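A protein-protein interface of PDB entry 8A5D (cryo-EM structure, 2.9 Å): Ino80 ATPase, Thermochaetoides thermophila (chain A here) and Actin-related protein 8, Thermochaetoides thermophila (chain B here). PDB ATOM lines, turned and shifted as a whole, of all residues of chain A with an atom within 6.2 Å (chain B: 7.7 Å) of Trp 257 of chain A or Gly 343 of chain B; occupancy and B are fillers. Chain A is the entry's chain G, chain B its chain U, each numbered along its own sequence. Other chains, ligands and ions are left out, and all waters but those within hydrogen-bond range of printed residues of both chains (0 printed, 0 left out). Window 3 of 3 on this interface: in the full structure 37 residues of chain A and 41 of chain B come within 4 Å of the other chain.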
ATOM      1  N   ASP A 252      29.209  -0.309  24.795  1.00  0.00           N
ATOM      2  CA  ASP A 252      28.750   1.059  24.425  1.00  0.00           C
ATOM      3  C   ASP A 252      27.220   1.121  24.278  1.00  0.00           C
ATOM      4  O   ASP A 252      26.619   2.120  24.712  1.00  0.00           O
ATOM      5  CB  ASP A 252      29.416   1.622  23.170  1.00  0.00           C
ATOM      6  CG  ASP A 252      29.670   3.132  23.247  1.00  0.00           C
ATOM      7  OD1 ASP A 252      29.151   3.806  24.166  1.00  0.00           O
ATOM      8  OD2 ASP A 252      30.434   3.645  22.398  1.00  0.00           O
ATOM      9  N   MET A 253      26.593   0.057  23.816  1.00  0.00           N
ATOM     10  CA  MET A 253      25.111  -0.069  23.778  1.00  0.00           C
ATOM     11  C   MET A 253      24.551  -0.179  25.192  1.00  0.00           C
ATOM     12  O   MET A 253      23.555   0.515  25.463  1.00  0.00           O
ATOM     13  CB  MET A 253      24.702  -1.253  22.916  1.00  0.00           C
ATOM     14  CG  MET A 253      23.288  -1.610  22.968  1.00  0.00           C
ATOM     15  SD  MET A 253      22.897  -2.669  24.400  1.00  0.00           S
ATOM     16  CE  MET A 253      23.814  -4.180  24.197  1.00  0.00           C
ATOM     17  N   MET A 254      25.219  -0.844  26.123  1.00  0.00           N
ATOM     18  CA  MET A 254      24.749  -0.868  27.548  1.00  0.00           C
ATOM     19  C   MET A 254      24.914   0.510  28.191  1.00  0.00           C
ATOM     20  O   MET A 254      23.975   0.962  28.924  1.00  0.00           O
ATOM     21  CB  MET A 254      25.483  -1.918  28.374  1.00  0.00           C
ATOM     22  CG  MET A 254      25.180  -3.327  27.882  1.00  0.00           C
ATOM     23  SD  MET A 254      23.400  -3.697  27.797  1.00  0.00           S
ATOM     24  CE  MET A 254      23.049  -3.891  29.546  1.00  0.00           C
ATOM     25  N   GLY A 255      25.968   1.223  27.820  1.00  0.00           N
ATOM     26  CA  GLY A 255      26.185   2.608  28.269  1.00  0.00           C
ATOM     27  C   GLY A 255      25.069   3.507  27.801  1.00  0.00           C
ATOM     28  O   GLY A 255      24.597   4.370  28.602  1.00  0.00           O
ATOM     29  N   PHE A 256      24.701   3.356  26.531  1.00  0.00           N
ATOM     30  CA  PHE A 256      23.671   4.186  25.867  1.00  0.00           C
ATOM     31  C   PHE A 256      22.378   4.116  26.670  1.00  0.00           C
ATOM     32  O   PHE A 256      21.803   5.177  26.949  1.00  0.00           O
ATOM     33  CB  PHE A 256      23.483   3.730  24.430  1.00  0.00           C
ATOM     34  CG  PHE A 256      22.350   4.384  23.708  1.00  0.00           C
ATOM     35  CD1 PHE A 256      21.076   3.864  23.814  1.00  0.00           C
ATOM     36  CD2 PHE A 256      22.571   5.523  22.945  1.00  0.00           C
ATOM     37  CE1 PHE A 256      20.033   4.488  23.158  1.00  0.00           C
ATOM     38  CE2 PHE A 256      21.524   6.145  22.287  1.00  0.00           C
ATOM     39  CZ  PHE A 256      20.254   5.623  22.398  1.00  0.00           C
ATOM     40  N   TRP A 257      21.936   2.918  27.019  1.00  0.00           N
ATOM     41  CA  TRP A 257      20.676   2.755  27.777  1.00  0.00           C
ATOM     42  C   TRP A 257      20.868   3.299  29.198  1.00  0.00           C
ATOM     43  O   TRP A 257      19.962   4.018  29.639  1.00  0.00           O
ATOM     44  CB  TRP A 257      20.166   1.311  27.760  1.00  0.00           C
ATOM     45  CG  TRP A 257      19.698   0.877  26.401  1.00  0.00           C
ATOM     46  CD1 TRP A 257      20.241  -0.130  25.659  1.00  0.00           C
ATOM     47  CD2 TRP A 257      18.618   1.404  25.605  1.00  0.00           C
ATOM     48  NE1 TRP A 257      19.596  -0.251  24.465  1.00  0.00           N
ATOM     49  CE2 TRP A 257      18.609   0.686  24.387  1.00  0.00           C
ATOM     50  CE3 TRP A 257      17.650   2.392  25.791  1.00  0.00           C
ATOM     51  CZ2 TRP A 257      17.691   0.929  23.361  1.00  0.00           C
ATOM     52  CZ3 TRP A 257      16.727   2.622  24.789  1.00  0.00           C
ATOM     53  CH2 TRP A 257      16.746   1.899  23.593  1.00  0.00           C
ATOM     54  N   LYS A 258      21.974   3.023  29.891  1.00  0.00           N
ATOM     55  CA  LYS A 258      22.170   3.554  31.266  1.00  0.00           C
ATOM     56  C   LYS A 258      22.077   5.098  31.289  1.00  0.00           C
ATOM     57  O   LYS A 258      21.772   5.610  32.374  1.00  0.00           O
ATOM     58  CB  LYS A 258      23.504   3.129  31.883  1.00  0.00           C
ATOM     59  CG  LYS A 258      23.629   1.669  32.266  1.00  0.00           C
ATOM     60  CD  LYS A 258      25.083   1.291  32.563  1.00  0.00           C
ATOM     61  CE  LYS A 258      25.340  -0.200  32.701  1.00  0.00           C
ATOM     62  NZ  LYS A 258      26.758  -0.549  32.433  1.00  0.00           N
ATOM     63  N   ARG A 259      22.390   5.835  30.217  1.00  0.00           N
ATOM     64  CA  ARG A 259      22.163   7.301  30.141  1.00  0.00           C
ATOM     65  C   ARG A 259      20.693   7.586  29.846  1.00  0.00           C
ATOM     66  O   ARG A 259      20.021   8.175  30.705  1.00  0.00           O
ATOM     67  CB  ARG A 259      22.987   7.978  29.054  1.00  0.00           C
ATOM     68  CG  ARG A 259      24.478   7.998  29.343  1.00  0.00           C
ATOM     69  CD  ARG A 259      25.223   9.013  28.478  1.00  0.00           C
ATOM     70  NE  ARG A 259      25.029   8.887  27.030  1.00  0.00           N
ATOM     71  CZ  ARG A 259      25.712   8.085  26.198  1.00  0.00           C
ATOM     72  NH1 ARG A 259      26.654   7.262  26.645  1.00  0.00           N
ATOM     73  NH2 ARG A 259      25.423   8.100  24.904  1.00  0.00           N
ATOM     74  N   ASN A 260      20.182   7.152  28.696  1.00  0.00           N
ATOM     75  CA  ASN A 260      18.820   7.520  28.205  1.00  0.00           C
ATOM     76  C   ASN A 260      17.726   6.994  29.150  1.00  0.00           C
ATOM     77  O   ASN A 260      16.873   7.794  29.545  1.00  0.00           O
ATOM     78  CB  ASN A 260      18.640   7.099  26.756  1.00  0.00           C
ATOM     79  CG  ASN A 260      19.554   7.908  25.851  1.00  0.00           C
ATOM     80  OD1 ASN A 260      19.198   9.009  25.439  1.00  0.00           O
ATOM     81  ND2 ASN A 260      20.747   7.405  25.554  1.00  0.00           N
ATOM     82  N   GLU A 261      17.799   5.748  29.609  1.00  0.00           N
ATOM     83  CA  GLU A 261      16.810   5.169  30.569  1.00  0.00           C
ATOM     84  C   GLU A 261      16.875   5.876  31.943  1.00  0.00           C
ATOM     85  O   GLU A 261      15.895   5.745  32.705  1.00  0.00           O
ATOM     86  CB  GLU A 261      17.027   3.657  30.695  1.00  0.00           C
ATOM     87  CG  GLU A 261      15.810   2.903  31.206  1.00  0.00           C
ATOM     88  CD  GLU A 261      15.965   1.392  31.300  1.00  0.00           C
ATOM     89  OE1 GLU A 261      15.252   0.784  32.119  1.00  0.00           O
ATOM     90  OE2 GLU A 261      16.788   0.824  30.552  1.00  0.00           O
ATOM     91  N   ARG A 262      17.950   6.617  32.253  1.00  0.00           N
ATOM     92  CA  ARG A 262      18.120   7.390  33.521  1.00  0.00           C
ATOM     93  C   ARG A 262      17.695   8.858  33.330  1.00  0.00           C
ATOM     94  O   ARG A 262      17.171   9.448  34.307  1.00  0.00           O
ATOM     95  CB  ARG A 262      19.570   7.259  34.001  1.00  0.00           C
ATOM     96  CG  ARG A 262      19.948   8.073  35.236  1.00  0.00           C
ATOM     97  CD  ARG A 262      20.660   9.384  34.920  1.00  0.00           C
ATOM     98  NE  ARG A 262      21.957   9.175  34.275  1.00  0.00           N
ATOM     99  CZ  ARG A 262      22.675  10.096  33.622  1.00  0.00           C
ATOM    100  NH1 ARG A 262      22.259  11.350  33.530  1.00  0.00           N
ATOM    101  NH2 ARG A 262      23.828   9.753  33.066  1.00  0.00           N
ATOM    102  N   ILE B 334      24.125  -5.002  10.403  1.00  0.00           N
ATOM    103  CA  ILE B 334      23.914  -5.647  11.723  1.00  0.00           C
ATOM    104  C   ILE B 334      22.934  -6.803  11.520  1.00  0.00           C
ATOM    105  O   ILE B 334      22.029  -6.719  10.676  1.00  0.00           O
ATOM    106  CB  ILE B 334      23.474  -4.605  12.769  1.00  0.00           C
ATOM    107  CG1 ILE B 334      23.300  -5.240  14.156  1.00  0.00           C
ATOM    108  CG2 ILE B 334      22.244  -3.849  12.306  1.00  0.00           C
ATOM    109  CD1 ILE B 334      23.250  -4.271  15.350  1.00  0.00           C
ATOM    110  N   GLU B 336      19.867  -9.431  12.479  1.00  0.00           N
ATOM    111  CA  GLU B 336      18.532  -9.326  13.151  1.00  0.00           C
ATOM    112  C   GLU B 336      18.665  -9.638  14.647  1.00  0.00           C
ATOM    113  O   GLU B 336      18.181  -8.841  15.445  1.00  0.00           O
ATOM    114  CB  GLU B 336      17.425 -10.184  12.536  1.00  0.00           C
ATOM    115  CG  GLU B 336      16.991  -9.656  11.156  1.00  0.00           C
ATOM    116  CD  GLU B 336      15.960 -10.439  10.329  1.00  0.00           C
ATOM    117  OE1 GLU B 336      15.904 -11.688  10.441  1.00  0.00           O
ATOM    118  OE2 GLU B 336      15.193  -9.793   9.569  1.00  0.00           O
ATOM    119  N   SER B 337      19.231 -10.754  15.050  1.00  0.00           N
ATOM    120  CA  SER B 337      19.324 -11.124  16.483  1.00  0.00           C
ATOM    121  C   SER B 337      20.185 -10.133  17.266  1.00  0.00           C
ATOM    122  O   SER B 337      19.910  -9.906  18.440  1.00  0.00           O
ATOM    123  CB  SER B 337      19.819 -12.527  16.613  1.00  0.00           C
ATOM    124  OG  SER B 337      18.771 -13.386  16.176  1.00  0.00           O
ATOM    125  N   MET B 338      21.225  -9.581  16.653  1.00  0.00           N
ATOM    126  CA  MET B 338      22.109  -8.646  17.366  1.00  0.00           C
ATOM    127  C   MET B 338      21.297  -7.388  17.609  1.00  0.00           C
ATOM    128  O   MET B 338      21.176  -6.967  18.769  1.00  0.00           O
ATOM    129  CB  MET B 338      23.370  -8.320  16.567  1.00  0.00           C
ATOM    130  CG  MET B 338      24.457  -7.732  17.435  1.00  0.00           C
ATOM    131  SD  MET B 338      25.068  -9.022  18.549  1.00  0.00           S
ATOM    132  CE  MET B 338      25.063  -8.171  20.121  1.00  0.00           C
ATOM    133  N   ALA B 339      20.703  -6.855  16.563  1.00  0.00           N
ATOM    134  CA  ALA B 339      19.836  -5.653  16.599  1.00  0.00           C
ATOM    135  C   ALA B 339      18.688  -5.858  17.625  1.00  0.00           C
ATOM    136  O   ALA B 339      18.440  -4.979  18.401  1.00  0.00           O
ATOM    137  CB  ALA B 339      19.354  -5.395  15.166  1.00  0.00           C
ATOM    138  N   ALA B 340      18.006  -6.997  17.667  1.00  0.00           N
ATOM    139  CA  ALA B 340      16.989  -7.292  18.697  1.00  0.00           C
ATOM    140  C   ALA B 340      17.531  -7.092  20.126  1.00  0.00           C
ATOM    141  O   ALA B 340      16.887  -6.387  20.927  1.00  0.00           O
ATOM    142  CB  ALA B 340      16.521  -8.697  18.540  1.00  0.00           C
ATOM    143  N   THR B 341      18.695  -7.627  20.472  1.00  0.00           N
ATOM    144  CA  THR B 341      19.231  -7.481  21.843  1.00  0.00           C
ATOM    145  C   THR B 341      19.592  -6.012  22.037  1.00  0.00           C
ATOM    146  O   THR B 341      19.499  -5.553  23.177  1.00  0.00           O
ATOM    147  CB  THR B 341      20.440  -8.379  22.133  1.00  0.00           C
ATOM    148  OG1 THR B 341      21.567  -8.047  21.299  1.00  0.00           O
ATOM    149  CG2 THR B 341      20.096  -9.834  21.935  1.00  0.00           C
ATOM    150  N   PHE B 342      20.071  -5.314  21.023  1.00  0.00           N
ATOM    151  CA  PHE B 342      20.464  -3.884  21.177  1.00  0.00           C
ATOM    152  C   PHE B 342      19.223  -3.019  21.385  1.00  0.00           C
ATOM    153  O   PHE B 342      19.359  -1.963  21.993  1.00  0.00           O
ATOM    154  CB  PHE B 342      21.215  -3.355  19.952  1.00  0.00           C
ATOM    155  CG  PHE B 342      22.690  -3.618  19.930  1.00  0.00           C
ATOM    156  CD1 PHE B 342      23.241  -4.684  20.611  1.00  0.00           C
ATOM    157  CD2 PHE B 342      23.520  -2.783  19.212  1.00  0.00           C
ATOM    158  CE1 PHE B 342      24.614  -4.862  20.618  1.00  0.00           C
ATOM    159  CE2 PHE B 342      24.884  -2.992  19.198  1.00  0.00           C
ATOM    160  CZ  PHE B 342      25.432  -4.024  19.912  1.00  0.00           C
ATOM    161  N   GLY B 343      18.073  -3.434  20.862  1.00  0.00           N
ATOM    162  CA  GLY B 343      16.770  -2.790  21.099  1.00  0.00           C
ATOM    163  C   GLY B 343      16.383  -2.912  22.559  1.00  0.00           C
ATOM    164  O   GLY B 343      15.945  -1.914  23.171  1.00  0.00           O
ATOM    165  N   ALA B 344      16.514  -4.105  23.091  1.00  0.00           N
ATOM    166  CA  ALA B 344      16.183  -4.434  24.484  1.00  0.00           C
ATOM    167  C   ALA B 344      17.172  -3.762  25.430  1.00  0.00           C
ATOM    168  O   ALA B 344      16.720  -3.282  26.491  1.00  0.00           O
ATOM    169  CB  ALA B 344      16.205  -5.935  24.670  1.00  0.00           C
ATOM    170  N   GLY B 345      18.463  -3.776  25.116  1.00  0.00           N
ATOM    171  CA  GLY B 345      19.540  -3.530  26.092  1.00  0.00           C
ATOM    172  C   GLY B 345      19.906  -4.787  26.864  1.00  0.00           C
ATOM    173  O   GLY B 345      20.083  -4.684  28.099  1.00  0.00           O
ATOM    174  N   TYR B 346      20.050  -5.914  26.163  1.00  0.00           N
ATOM    175  CA  TYR B 346      20.439  -7.227  26.742  1.00  0.00           C
ATOM    176  C   TYR B 346      21.846  -7.596  26.293  1.00  0.00           C
ATOM    177  O   TYR B 346      22.173  -7.507  25.115  1.00  0.00           O
ATOM    178  CB  TYR B 346      19.483  -8.346  26.330  1.00  0.00           C
ATOM    179  CG  TYR B 346      18.060  -8.270  26.836  1.00  0.00           C
ATOM    180  CD1 TYR B 346      17.713  -7.573  27.981  1.00  0.00           C
ATOM    181  CD2 TYR B 346      17.052  -8.956  26.173  1.00  0.00           C
ATOM    182  CE1 TYR B 346      16.404  -7.556  28.443  1.00  0.00           C
ATOM    183  CE2 TYR B 346      15.740  -8.947  26.617  1.00  0.00           C
ATOM    184  CZ  TYR B 346      15.411  -8.244  27.760  1.00  0.00           C
ATOM    185  OH  TYR B 346      14.108  -8.232  28.177  1.00  0.00           O
ATOM    186  N   MET B 664      13.518 -14.396  24.066  1.00  0.00           N
ATOM    187  CA  MET B 664      12.882 -13.121  23.701  1.00  0.00           C
ATOM    188  C   MET B 664      12.200 -13.317  22.346  1.00  0.00           C
ATOM    189  O   MET B 664      12.877 -13.666  21.362  1.00  0.00           O
ATOM    190  CB  MET B 664      13.979 -12.058  23.638  1.00  0.00           C
ATOM    191  CG  MET B 664      13.549 -10.737  23.053  1.00  0.00           C
ATOM    192  SD  MET B 664      14.915  -9.547  23.151  1.00  0.00           S
ATOM    193  CE  MET B 664      14.207  -8.219  22.182  1.00  0.00           C
ATOM    194  N   ALA B 700      10.605  -6.113  24.147  1.00  0.00           N
ATOM    195  CA  ALA B 700      11.422  -5.527  25.226  1.00  0.00           C
ATOM    196  C   ALA B 700      11.123  -4.037  25.400  1.00  0.00           C
ATOM    197  O   ALA B 700      10.770  -3.379  24.392  1.00  0.00           O
ATOM    198  CB  ALA B 700      12.870  -5.744  24.904  1.00  0.00           C
ATOM    199  N   ARG B 701      11.262  -3.540  26.639  1.00  0.00           N
ATOM    200  CA  ARG B 701      11.027  -2.127  27.060  1.00  0.00           C
ATOM    201  C   ARG B 701       9.793  -1.553  26.319  1.00  0.00           C
ATOM    202  O   ARG B 701       9.822  -0.394  25.833  1.00  0.00           O
ATOM    203  CB  ARG B 701      12.340  -1.320  26.981  1.00  0.00           C
ATOM    204  CG  ARG B 701      12.942  -1.148  25.595  1.00  0.00           C
ATOM    205  CD  ARG B 701      14.131  -0.208  25.619  1.00  0.00           C
ATOM    206  NE  ARG B 701      15.224  -0.780  26.394  1.00  0.00           N
ATOM    207  CZ  ARG B 701      15.845  -0.191  27.401  1.00  0.00           C
ATOM    208  NH1 ARG B 701      15.492   1.020  27.794  1.00  0.00           N
ATOM    209  NH2 ARG B 701      16.830  -0.811  28.028  1.00  0.00           N
ATOM    210  N   MET B 703       8.110  -1.927  23.702  1.00  0.00           N
ATOM    211  CA  MET B 703       8.010  -1.729  22.230  1.00  0.00           C
ATOM    212  C   MET B 703       7.052  -2.738  21.600  1.00  0.00           C
ATOM    213  O   MET B 703       6.803  -3.806  22.171  1.00  0.00           O
ATOM    214  CB  MET B 703       9.370  -1.873  21.557  1.00  0.00           C
ATOM    215  CG  MET B 703      10.221  -0.672  21.809  1.00  0.00           C
ATOM    216  SD  MET B 703      11.765  -0.727  20.938  1.00  0.00           S
ATOM    217  CE  MET B 703      12.743  -1.713  22.070  1.00  0.00           C
ATOM    218  N   VAL B 707       8.994  -3.655  15.839  1.00  0.00           N
ATOM    219  CA  VAL B 707      10.005  -2.560  15.731  1.00  0.00           C
ATOM    220  C   VAL B 707      11.184  -2.740  16.688  1.00  0.00           C
ATOM    221  O   VAL B 707      12.101  -1.882  16.590  1.00  0.00           O
ATOM    222  CB  VAL B 707       9.371  -1.184  15.957  1.00  0.00           C
ATOM    223  CG1 VAL B 707       8.177  -1.019  15.026  1.00  0.00           C
ATOM    224  CG2 VAL B 707       9.050  -0.924  17.461  1.00  0.00           C
ATOM    225  N   VAL B 708      11.255  -3.771  17.521  1.00  0.00           N
ATOM    226  CA  VAL B 708      12.407  -3.938  18.464  1.00  0.00           C
ATOM    227  C   VAL B 708      13.704  -3.957  17.655  1.00  0.00           C
ATOM    228  O   VAL B 708      14.703  -3.348  18.122  1.00  0.00           O
ATOM    229  CB  VAL B 708      12.338  -5.207  19.326  1.00  0.00           C
ATOM    230  CG1 VAL B 708      13.468  -5.193  20.323  1.00  0.00           C
ATOM    231  CG2 VAL B 708      11.032  -5.278  20.074  1.00  0.00           C
ATOM    232  N   VAL B 709      13.697  -4.625  16.502  1.00  0.00           N
ATOM    233  CA  VAL B 709      14.916  -4.826  15.687  1.00  0.00           C
ATOM    234  C   VAL B 709      15.330  -3.483  15.097  1.00  0.00           C
ATOM    235  O   VAL B 709      16.521  -3.129  15.183  1.00  0.00           O
ATOM    236  CB  VAL B 709      14.730  -5.904  14.612  1.00  0.00           C
ATOM    237  CG1 VAL B 709      15.963  -6.020  13.729  1.00  0.00           C
ATOM    238  CG2 VAL B 709      14.425  -7.249  15.274  1.00  0.00           C
ATOM    239  N   TRP B 710      14.407  -2.711  14.550  1.00  0.00           N
ATOM    240  CA  TRP B 710      14.775  -1.385  13.962  1.00  0.00           C
ATOM    241  C   TRP B 710      15.278  -0.456  15.050  1.00  0.00           C
ATOM    242  O   TRP B 710      16.253   0.211  14.814  1.00  0.00           O
ATOM    243  CB  TRP B 710      13.601  -0.829  13.206  1.00  0.00           C
ATOM    244  CG  TRP B 710      13.887   0.392  12.451  1.00  0.00           C
ATOM    245  CD1 TRP B 710      14.032   0.457  11.119  1.00  0.00           C
ATOM    246  CD2 TRP B 710      13.929   1.745  12.935  1.00  0.00           C
ATOM    247  NE1 TRP B 710      14.267   1.750  10.732  1.00  0.00           N
ATOM    248  CE2 TRP B 710      14.179   2.567  11.812  1.00  0.00           C
ATOM    249  CE3 TRP B 710      13.783   2.350  14.186  1.00  0.00           C
ATOM    250  CZ2 TRP B 710      14.313   3.944  11.900  1.00  0.00           C
ATOM    251  CZ3 TRP B 710      13.937   3.712  14.275  1.00  0.00           C
ATOM    252  CH2 TRP B 710      14.208   4.492  13.152  1.00  0.00           C
ATOM    253  N   LYS B 711      14.669  -0.449  16.231  1.00  0.00           N
ATOM    254  CA  LYS B 711      15.160   0.381  17.345  1.00  0.00           C
ATOM    255  C   LYS B 711      16.607   0.004  17.647  1.00  0.00           C
ATOM    256  O   LYS B 711      17.449   0.955  17.669  1.00  0.00           O
ATOM    257  CB  LYS B 711      14.275   0.240  18.567  1.00  0.00           C
ATOM    258  CG  LYS B 711      14.777   0.994  19.798  1.00  0.00           C
ATOM    259  CD  LYS B 711      14.780   2.514  19.662  1.00  0.00           C
ATOM    260  CE  LYS B 711      13.400   3.070  19.425  1.00  0.00           C
ATOM    261  NZ  LYS B 711      13.345   4.534  19.648  1.00  0.00           N
ATOM    262  N   GLY B 712      16.938  -1.286  17.772  1.00  0.00           N
ATOM    263  CA  GLY B 712      18.351  -1.740  17.961  1.00  0.00           C
ATOM    264  C   GLY B 712      19.333  -1.280  16.850  1.00  0.00           C
ATOM    265  O   GLY B 712      20.415  -0.761  17.163  1.00  0.00           O
ATOM    266  N   ALA B 713      18.936  -1.384  15.582  1.00  0.00           N
ATOM    267  CA  ALA B 713      19.715  -0.911  14.424  1.00  0.00           C
ATOM    268  C   ALA B 713      19.968   0.592  14.530  1.00  0.00           C
ATOM    269  O   ALA B 713      21.088   1.055  14.169  1.00  0.00           O
ATOM    270  CB  ALA B 713      19.017  -1.233  13.121  1.00  0.00           C
ATOM    271  N   SER B 714      19.002   1.369  15.012  1.00  0.00           N
ATOM    272  CA  SER B 714      19.141   2.842  15.106  1.00  0.00           C
ATOM    273  C   SER B 714      20.101   3.160  16.248  1.00  0.00           C
ATOM    274  O   SER B 714      20.879   4.169  16.033  1.00  0.00           O
ATOM    275  CB  SER B 714      17.836   3.505  15.277  1.00  0.00           C
ATOM    276  OG  SER B 714      17.375   3.359  16.615  1.00  0.00           O
ATOM    277  N   VAL B 715      20.138   2.351  17.336  1.00  0.00           N
ATOM    278  CA  VAL B 715      21.130   2.610  18.425  1.00  0.00           C
ATOM    279  C   VAL B 715      22.530   2.324  17.857  1.00  0.00           C
ATOM    280  O   VAL B 715      23.481   3.068  18.155  1.00  0.00           O
ATOM    281  CB  VAL B 715      20.892   1.749  19.666  1.00  0.00           C
ATOM    282  CG1 VAL B 715      22.033   1.826  20.660  1.00  0.00           C
ATOM    283  CG2 VAL B 715      19.581   2.050  20.343  1.00  0.00           C
ATOM    284  N   PHE B 716      22.679   1.280  17.040  1.00  0.00           N
ATOM    285  CA  PHE B 716      23.972   0.880  16.436  1.00  0.00           C
ATOM    286  C   PHE B 716      24.487   1.985  15.521  1.00  0.00           C
ATOM    287  O   PHE B 716      25.715   2.172  15.452  1.00  0.00           O
ATOM    288  CB  PHE B 716      23.805  -0.453  15.725  1.00  0.00           C
ATOM    289  CG  PHE B 716      24.975  -0.962  14.919  1.00  0.00           C
ATOM    290  CD1 PHE B 716      26.065  -1.531  15.558  1.00  0.00           C
ATOM    291  CD2 PHE B 716      24.938  -0.954  13.525  1.00  0.00           C
ATOM    292  CE1 PHE B 716      27.082  -2.112  14.827  1.00  0.00           C
ATOM    293  CE2 PHE B 716      25.959  -1.522  12.791  1.00  0.00           C
ATOM    294  CZ  PHE B 716      27.025  -2.103  13.451  1.00  0.00           C
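The guanidinium group of Arg 701 of chain B lies within hydrogen-bond range of the backbone carbonyl oxygen of Ala 344 of chain B (2.9 Å). The side-chain amide nitrogen (ND2) of Asn 260 of chain A sits at hydrogen-bond distance from the backbone carbonyl oxygen (O) of Phe 256 of chain A (2.8 Å). The backbone NH of Tyr 346 of chain B lies within hydrogen-bond range of the backbone carbonyl oxygen of Thr 341 of chain B, 3.1 Å away. O of Gly 343 of chain B lies within hydrogen-bond range of NE of Arg 701 of chain B, at 3.5 Å.
Of the 26 printed residues of chain B, 6 touch a printed residue of chain A. Hydrophobic or aromatic side chains of chain B within 4 Å of the printed part of chain A: Phe 342 and Val 715. Among the printed residues, 11 pairs touch across the chains. Among the printed residues, Asp or Glu carboxylates within 4 Å of a Lys or Arg side-chain nitrogen of the other chain: Glu 261 of chain A with Arg 701 of chain B (3.0 Å).
The side-chain carboxylate (OE2) of Glu 261 of chain A lies within salt-bridge range of the guanidinium group (NH2) of Arg 701 of chain B, at 3.0 Å. SD of Met 254 of chain A lies close to O of Gly 345 of chain B, 3.5 Å away. NE1 of Trp 257 of chain A lies within hydrogen-bond range of O of Phe 342 of chain B (3.0 Å).
Of the printed residues of chain B, Met 254 of chain A touches Gly 345. Of the printed residues of chain B, Phe 256 of chain A touches Val 715. Trp 257 of chain A touches just these residues of chain B: Phe 342, Gly 343, Gly 345, Arg 701 and Val 715. Of chain A, only Trp 257 comes within 4 Å of Gly 343 of chain B. Of the printed residues of chain A, Arg 701 of chain B touches Trp 257 and Glu 261. Of the printed residues of chain A, Val 715 of chain B touches Phe 256 (3.8 Å) and Trp 257 (3.7 Å). The nearest printed residue of chain B that does not touch Trp 257 of chain A is Lys 711 of chain B (4.4 Å).
Among the printed residues, merely in contact across the chains: Trp 257 of chain A with Arg 701 of chain B, Trp 257 of chain A with Gly 343 of chain B, Trp 257 of chain A with Gly 345 of chain B, Met 253 of chain A with Phe 342 of chain B, Trp 257 of chain A with Val 715 of chain B, Phe 256 of chain A with Val 715 of chain B, Met 253 of chain A with Tyr 346 of chain B and Met 253 of chain A with Gly 345 of chain B.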
